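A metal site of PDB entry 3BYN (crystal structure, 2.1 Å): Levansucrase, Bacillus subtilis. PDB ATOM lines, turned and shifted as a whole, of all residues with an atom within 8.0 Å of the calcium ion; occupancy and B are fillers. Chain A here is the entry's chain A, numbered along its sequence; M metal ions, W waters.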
ATOM      1  N   GLN A 226      14.890  33.340  -4.756  1.00  0.00           N
ATOM      2  CA  GLN A 226      15.400  31.978  -4.563  1.00  0.00           C
ATOM      3  C   GLN A 226      16.865  31.891  -4.992  1.00  0.00           C
ATOM      4  O   GLN A 226      17.247  32.453  -6.015  1.00  0.00           O
ATOM      5  CB  GLN A 226      14.561  30.968  -5.362  1.00  0.00           C
ATOM      6  CG  GLN A 226      14.731  29.505  -4.923  1.00  0.00           C
ATOM      7  CD  GLN A 226      14.079  28.520  -5.878  1.00  0.00           C
ATOM      8  OE1 GLN A 226      14.209  28.623  -7.099  1.00  0.00           O
ATOM      9  NE2 GLN A 226      13.371  27.538  -5.320  1.00  0.00           N
ATOM     10  N   PHE A 231      17.064  25.382  -4.244  1.00  0.00           N
ATOM     11  CA  PHE A 231      16.806  24.429  -5.316  1.00  0.00           C
ATOM     12  C   PHE A 231      17.341  23.042  -4.954  1.00  0.00           C
ATOM     13  O   PHE A 231      16.652  22.042  -5.135  1.00  0.00           O
ATOM     14  CB  PHE A 231      17.442  24.934  -6.617  1.00  0.00           C
ATOM     15  CG  PHE A 231      17.175  24.072  -7.829  1.00  0.00           C
ATOM     16  CD1 PHE A 231      15.880  23.730  -8.196  1.00  0.00           C
ATOM     17  CD2 PHE A 231      18.244  23.638  -8.622  1.00  0.00           C
ATOM     18  CE1 PHE A 231      15.649  22.947  -9.332  1.00  0.00           C
ATOM     19  CE2 PHE A 231      18.010  22.862  -9.765  1.00  0.00           C
ATOM     20  CZ  PHE A 231      16.718  22.520 -10.118  1.00  0.00           C
ATOM     21  N   GLU A 234      15.366  21.116  -2.358  1.00  0.00           N
ATOM     22  CA  GLU A 234      14.189  20.429  -2.907  1.00  0.00           C
ATOM     23  C   GLU A 234      14.557  19.087  -3.569  1.00  0.00           C
ATOM     24  O   GLU A 234      13.702  18.217  -3.744  1.00  0.00           O
ATOM     25  CB  GLU A 234      13.487  21.315  -3.952  1.00  0.00           C
ATOM     26  CG  GLU A 234      13.018  22.691  -3.465  1.00  0.00           C
ATOM     27  CD  GLU A 234      11.720  22.662  -2.650  1.00  0.00           C
ATOM     28  OE1 GLU A 234      11.100  21.588  -2.480  1.00  0.00           O
ATOM     29  OE2 GLU A 234      11.304  23.753  -2.185  1.00  0.00           O
ATOM     30  N   SER A 239      13.095  17.195  -8.557  1.00  0.00           N
ATOM     31  CA  SER A 239      11.969  17.684  -7.746  1.00  0.00           C
ATOM     32  C   SER A 239      10.853  18.277  -8.600  1.00  0.00           C
ATOM     33  O   SER A 239       9.713  18.383  -8.156  1.00  0.00           O
ATOM     34  CB  SER A 239      12.447  18.711  -6.708  1.00  0.00           C
ATOM     35  OG  SER A 239      12.723  19.963  -7.304  1.00  0.00           O
ATOM     36  N   GLY A 240      11.193  18.674  -9.825  1.00  0.00           N
ATOM     37  CA  GLY A 240      10.260  19.370 -10.713  1.00  0.00           C
ATOM     38  C   GLY A 240      10.321  20.879 -10.562  1.00  0.00           C
ATOM     39  O   GLY A 240       9.660  21.607 -11.297  1.00  0.00           O
ATOM     40  N   ASP A 241      11.106  21.348  -9.597  1.00  0.00           N
ATOM     41  CA  ASP A 241      11.306  22.781  -9.403  1.00  0.00           C
ATOM     42  C   ASP A 241      12.135  23.361 -10.549  1.00  0.00           C
ATOM     43  O   ASP A 241      12.914  22.656 -11.182  1.00  0.00           O
ATOM     44  CB  ASP A 241      11.976  23.072  -8.054  1.00  0.00           C
ATOM     45  CG  ASP A 241      11.693  24.487  -7.547  1.00  0.00           C
ATOM     46  OD1 ASP A 241      10.734  25.135  -8.019  1.00  0.00           O
ATOM     47  OD2 ASP A 241      12.445  24.958  -6.669  1.00  0.00           O
ATOM     48  N   ASN A 242      11.930  24.640 -10.834  1.00  0.00           N
ATOM     49  CA  ASN A 242      12.662  25.332 -11.874  1.00  0.00           C
ATOM     50  C   ASN A 242      13.304  26.581 -11.285  1.00  0.00           C
ATOM     51  O   ASN A 242      12.645  27.617 -11.123  1.00  0.00           O
ATOM     52  CB  ASN A 242      11.735  25.686 -13.056  1.00  0.00           C
ATOM     53  CG  ASN A 242      12.479  26.280 -14.240  1.00  0.00           C
ATOM     54  OD1 ASN A 242      13.716  26.312 -14.284  1.00  0.00           O
ATOM     55  ND2 ASN A 242      11.726  26.756 -15.228  1.00  0.00           N
ATOM     56  N   HIS A 243      14.587  26.477 -10.941  1.00  0.00           N
ATOM     57  CA  HIS A 243      15.327  27.606 -10.377  1.00  0.00           C
ATOM     58  C   HIS A 243      15.860  28.502 -11.487  1.00  0.00           C
ATOM     59  O   HIS A 243      16.524  28.035 -12.421  1.00  0.00           O
ATOM     60  CB  HIS A 243      16.458  27.152  -9.452  1.00  0.00           C
ATOM     61  CG  HIS A 243      17.364  28.266  -9.029  1.00  0.00           C
ATOM     62  ND1 HIS A 243      16.920  29.330  -8.273  1.00  0.00           N
ATOM     63  CD2 HIS A 243      18.673  28.490  -9.280  1.00  0.00           C
ATOM     64  CE1 HIS A 243      17.919  30.174  -8.081  1.00  0.00           C
ATOM     65  NE2 HIS A 243      18.993  29.691  -8.677  1.00  0.00           N
ATOM     66  N   THR A 244      15.557  29.784 -11.363  1.00  0.00           N
ATOM     67  CA  THR A 244      15.996  30.771 -12.329  1.00  0.00           C
ATOM     68  C   THR A 244      16.533  32.002 -11.626  1.00  0.00           C
ATOM     69  O   THR A 244      16.020  32.415 -10.588  1.00  0.00           O
ATOM     70  CB  THR A 244      14.851  31.202 -13.286  1.00  0.00           C
ATOM     71  OG1 THR A 244      13.976  32.106 -12.610  1.00  0.00           O
ATOM     72  CG2 THR A 244      14.043  29.996 -13.795  1.00  0.00           C
ATOM     73  N   ALA A 263      13.524  35.737 -12.099  1.00  0.00           N
ATOM     74  CA  ALA A 263      13.862  35.111 -10.823  1.00  0.00           C
ATOM     75  C   ALA A 263      12.723  34.228 -10.340  1.00  0.00           C
ATOM     76  O   ALA A 263      11.776  33.938 -11.076  1.00  0.00           O
ATOM     77  CB  ALA A 263      14.210  36.180  -9.777  1.00  0.00           C
ATOM     78  N   ASN A 264      12.832  33.800  -9.098  1.00  0.00           N
ATOM     79  CA  ASN A 264      11.751  33.148  -8.383  1.00  0.00           C
ATOM     80  C   ASN A 264      11.701  33.747  -6.990  1.00  0.00           C
ATOM     81  O   ASN A 264      12.729  34.209  -6.484  1.00  0.00           O
ATOM     82  CB  ASN A 264      11.951  31.633  -8.327  1.00  0.00           C
ATOM     83  CG  ASN A 264      12.070  31.010  -9.714  1.00  0.00           C
ATOM     84  OD1 ASN A 264      13.145  31.000 -10.314  1.00  0.00           O
ATOM     85  ND2 ASN A 264      10.953  30.498 -10.234  1.00  0.00           N
ATOM     86  N   THR A 265      10.522  33.768  -6.380  1.00  0.00           N
ATOM     87  CA  THR A 265      10.351  34.368  -5.052  1.00  0.00           C
ATOM     88  C   THR A 265      11.159  33.622  -3.987  1.00  0.00           C
ATOM     89  O   THR A 265      11.583  32.482  -4.197  1.00  0.00           O
ATOM     90  CB  THR A 265       8.872  34.424  -4.619  1.00  0.00           C
ATOM     91  OG1 THR A 265       8.353  33.095  -4.551  1.00  0.00           O
ATOM     92  CG2 THR A 265       8.041  35.259  -5.588  1.00  0.00           C
ATOM     93  N   TYR A 271       6.599  32.367  -1.038  1.00  0.00           N
ATOM     94  CA  TYR A 271       7.404  31.272  -1.537  1.00  0.00           C
ATOM     95  C   TYR A 271       6.523  30.176  -2.141  1.00  0.00           C
ATOM     96  O   TYR A 271       5.313  30.141  -1.907  1.00  0.00           O
ATOM     97  CB  TYR A 271       8.298  30.698  -0.427  1.00  0.00           C
ATOM     98  CG  TYR A 271       9.481  29.896  -0.927  1.00  0.00           C
ATOM     99  CD1 TYR A 271      10.300  30.403  -1.951  1.00  0.00           C
ATOM    100  CD2 TYR A 271       9.794  28.650  -0.392  1.00  0.00           C
ATOM    101  CE1 TYR A 271      11.393  29.678  -2.425  1.00  0.00           C
ATOM    102  CE2 TYR A 271      10.899  27.921  -0.862  1.00  0.00           C
ATOM    103  CZ  TYR A 271      11.684  28.443  -1.886  1.00  0.00           C
ATOM    104  OH  TYR A 271      12.772  27.747  -2.360  1.00  0.00           O
ATOM    105  N   GLN A 272       7.151  29.294  -2.912  1.00  0.00           N
ATOM    106  CA  GLN A 272       6.524  28.083  -3.413  1.00  0.00           C
ATOM    107  C   GLN A 272       6.133  27.176  -2.242  1.00  0.00           C
ATOM    108  O   GLN A 272       6.665  27.308  -1.138  1.00  0.00           O
ATOM    109  CB  GLN A 272       7.480  27.351  -4.363  1.00  0.00           C
ATOM    110  CG  GLN A 272       8.759  26.815  -3.696  1.00  0.00           C
ATOM    111  CD  GLN A 272       9.844  26.477  -4.693  1.00  0.00           C
ATOM    112  OE1 GLN A 272      10.008  27.152  -5.719  1.00  0.00           O
ATOM    113  NE2 GLN A 272      10.627  25.441  -4.396  1.00  0.00           N
ATOM    114  N   GLY A 273       5.202  26.264  -2.499  1.00  0.00           N
ATOM    115  CA  GLY A 273       4.781  25.302  -1.487  1.00  0.00           C
ATOM    116  C   GLY A 273       3.294  25.013  -1.533  1.00  0.00           C
ATOM    117  O   GLY A 273       2.540  25.653  -2.287  1.00  0.00           O
ATOM    118  N   THR A 305       2.755  21.146  -9.941  1.00  0.00           N
ATOM    119  CA  THR A 305       3.333  22.178 -10.819  1.00  0.00           C
ATOM    120  C   THR A 305       3.005  23.585 -10.286  1.00  0.00           C
ATOM    121  O   THR A 305       3.891  24.453 -10.198  1.00  0.00           O
ATOM    122  CB  THR A 305       2.834  22.010 -12.279  1.00  0.00           C
ATOM    123  OG1 THR A 305       3.191  20.708 -12.750  1.00  0.00           O
ATOM    124  CG2 THR A 305       3.460  23.057 -13.205  1.00  0.00           C
ATOM    125  N   ALA A 306       1.734  23.791  -9.923  1.00  0.00           N
ATOM    126  CA  ALA A 306       1.256  25.065  -9.371  1.00  0.00           C
ATOM    127  C   ALA A 306       1.925  25.406  -8.031  1.00  0.00           C
ATOM    128  O   ALA A 306       2.262  26.561  -7.772  1.00  0.00           O
ATOM    129  CB  ALA A 306      -0.259  25.036  -9.224  1.00  0.00           C
ATOM    130  N   GLU A 307       2.108  24.396  -7.184  1.00  0.00           N
ATOM    131  CA  GLU A 307       2.781  24.580  -5.898  1.00  0.00           C
ATOM    132  C   GLU A 307       4.221  25.077  -6.066  1.00  0.00           C
ATOM    133  O   GLU A 307       4.666  25.962  -5.342  1.00  0.00           O
ATOM    134  CB  GLU A 307       2.724  23.300  -5.069  1.00  0.00           C
ATOM    135  CG  GLU A 307       1.327  22.996  -4.510  1.00  0.00           C
ATOM    136  CD  GLU A 307       1.147  21.552  -4.039  1.00  0.00           C
ATOM    137  OE1 GLU A 307       1.985  20.684  -4.374  1.00  0.00           O
ATOM    138  OE2 GLU A 307       0.156  21.296  -3.325  1.00  0.00           O
ATOM    139  N   LEU A 308       4.916  24.515  -7.063  1.00  0.00           N
ATOM    140  CA  LEU A 308       6.314  24.854  -7.339  1.00  0.00           C
ATOM    141  C   LEU A 308       6.485  26.168  -8.109  1.00  0.00           C
ATOM    142  O   LEU A 308       7.572  26.741  -8.131  1.00  0.00           O
ATOM    143  CB  LEU A 308       6.979  23.721  -8.138  1.00  0.00           C
ATOM    144  CG  LEU A 308       7.228  22.385  -7.418  1.00  0.00           C
ATOM    145  CD1 LEU A 308       7.279  21.240  -8.426  1.00  0.00           C
ATOM    146  CD2 LEU A 308       8.499  22.449  -6.583  1.00  0.00           C
ATOM    147  N   ALA A 309       5.407  26.624  -8.734  1.00  0.00           N
ATOM    148  CA  ALA A 309       5.433  27.814  -9.580  1.00  0.00           C
ATOM    149  C   ALA A 309       5.465  29.087  -8.743  1.00  0.00           C
ATOM    150  O   ALA A 309       4.491  29.415  -8.063  1.00  0.00           O
ATOM    151  CB  ALA A 309       4.232  27.811 -10.514  1.00  0.00           C
ATOM    152  N   ASN A 310       6.596  29.768  -8.765  1.00  0.00           N
ATOM    153  CA  ASN A 310       6.769  31.044  -8.071  1.00  0.00           C
ATOM    154  C   ASN A 310       7.715  31.967  -8.844  1.00  0.00           C
ATOM    155  O   ASN A 310       8.610  32.592  -8.254  1.00  0.00           O
ATOM    156  CB  ASN A 310       7.248  30.822  -6.620  1.00  0.00           C
ATOM    157  CG  ASN A 310       8.669  30.282  -6.525  1.00  0.00           C
ATOM    158  OD1 ASN A 310       9.125  29.565  -7.414  1.00  0.00           O
ATOM    159  ND2 ASN A 310       9.368  30.615  -5.454  1.00  0.00           N
ATOM    160  N   GLY A 311       7.516  32.035 -10.153  1.00  0.00           N
ATOM    161  CA  GLY A 311       8.290  32.943 -11.000  1.00  0.00           C
ATOM    162  C   GLY A 311       8.144  34.381 -10.556  1.00  0.00           C
ATOM    163  O   GLY A 311       7.137  34.753  -9.936  1.00  0.00           O
ATOM    164  N   ASN A 335       3.128  33.294  -8.915  1.00  0.00           N
ATOM    165  CA  ASN A 335       2.801  32.119  -8.091  1.00  0.00           C
ATOM    166  C   ASN A 335       1.575  31.344  -8.603  1.00  0.00           C
ATOM    167  O   ASN A 335       0.549  31.959  -8.949  1.00  0.00           O
ATOM    168  CB  ASN A 335       2.566  32.485  -6.631  1.00  0.00           C
ATOM    169  CG  ASN A 335       3.743  33.208  -6.017  1.00  0.00           C
ATOM    170  OD1 ASN A 335       3.985  34.383  -6.297  1.00  0.00           O
ATOM    171  ND2 ASN A 335       4.464  32.512  -5.144  1.00  0.00           N
ATOM    172  N   THR A 338       3.033  29.985 -13.274  1.00  0.00           N
ATOM    173  CA  THR A 338       4.239  29.431 -13.891  1.00  0.00           C
ATOM    174  C   THR A 338       5.479  29.734 -13.058  1.00  0.00           C
ATOM    175  O   THR A 338       5.504  30.699 -12.288  1.00  0.00           O
ATOM    176  CB  THR A 338       4.440  29.934 -15.349  1.00  0.00           C
ATOM    177  OG1 THR A 338       5.645  29.365 -15.893  1.00  0.00           O
ATOM    178  CG2 THR A 338       4.510  31.452 -15.412  1.00  0.00           C
ATOM    179  N   ASP A 339       6.490  28.888 -13.224  1.00  0.00           N
ATOM    180  CA  ASP A 339       7.780  29.028 -12.557  1.00  0.00           C
ATOM    181  C   ASP A 339       8.766  29.786 -13.450  1.00  0.00           C
ATOM    182  O   ASP A 339       9.907  30.065 -13.036  1.00  0.00           O
ATOM    183  CB  ASP A 339       8.343  27.646 -12.245  1.00  0.00           C
ATOM    184  CG  ASP A 339       9.018  27.572 -10.876  1.00  0.00           C
ATOM    185  OD1 ASP A 339       8.963  28.566 -10.116  1.00  0.00           O
ATOM    186  OD2 ASP A 339       9.609  26.518 -10.562  1.00  0.00           O
ATOM    187  N   GLU A 340       8.336  30.123 -14.663  1.00  0.00           N
ATOM    188  CA  GLU A 340       9.239  30.651 -15.672  1.00  0.00           C
ATOM    189  C   GLU A 340       8.668  31.839 -16.447  1.00  0.00           C
ATOM    190  O   GLU A 340       7.934  31.658 -17.428  1.00  0.00           O
ATOM    191  CB  GLU A 340       9.673  29.543 -16.627  1.00  0.00           C
ATOM    192  CG  GLU A 340      10.936  29.867 -17.417  1.00  0.00           C
ATOM    193  CD  GLU A 340      11.275  28.771 -18.408  1.00  0.00           C
ATOM    194  OE1 GLU A 340      10.697  28.775 -19.521  1.00  0.00           O
ATOM    195  OE2 GLU A 340      12.103  27.915 -18.057  1.00  0.00           O
HETATM  196 CA    CA M   1       9.792  27.327  -8.039  1.00  0.00          CA
HETATM  197  O   HOH W   1      12.028  28.132  -8.616  1.00  0.00           O
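OD2 of Asp 339 lies close to N of Asn 242 (3.0 Å). The side-chain carboxylate (OD2) of Asp 241 sits at hydrogen-bond distance from the side-chain amide nitrogen (NE2) of Gln 226, 3.1 Å away. ND2 of Asn 264 lies close to OD1 of Asn 310 (3.5 Å). The backbone NH of Asp 241 is in hydrogen-bond range of the side-chain hydroxyl of Ser 239 (3.1 Å). The side-chain amide nitrogen (NE2) of Gln 226 sits close to the side-chain amide oxygen (OE1) of Gln 272, at 3.4 Å. ND2 of Asn 310 sits at hydrogen-bond distance from OG1 of Thr 265, 2.8 Å away. The side-chain amide nitrogen (ND2) of Asn 264 sits at hydrogen-bond distance from the backbone carbonyl oxygen (O) of Asp 339, at 3.0 Å. The side-chain carboxylate of Glu 234 lies within hydrogen-bond range of the side-chain amide nitrogen of Gln 272, 2.9 Å away.
Along chain A the residues within 4 Å of the calcium ion span positions 241 to 339. The nearest printed residue that does not touch the calcium ion is Asn 264 (4.03 Å).
The calcium ion is bound by O of Leu 308 (2.3 Å), OE1 of Gln 272 (2.3 Å), OD1 of Asp 241 (2.4 Å), OD1 of Asn 310 (2.4 Å), water W1 (2.4 Å), OD1 of Asp 339 (2.6 Å) and OD2 of Asp 339 (2.7 Å). The calcium ion has seven donor atoms within binding distance.
Water W1 lies within hydrogen-bond range of O of Asn 242 (2.6 Å), OE1 of Gln 226 (2.7 Å) and ND2 of Asn 264 (3.1 Å).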
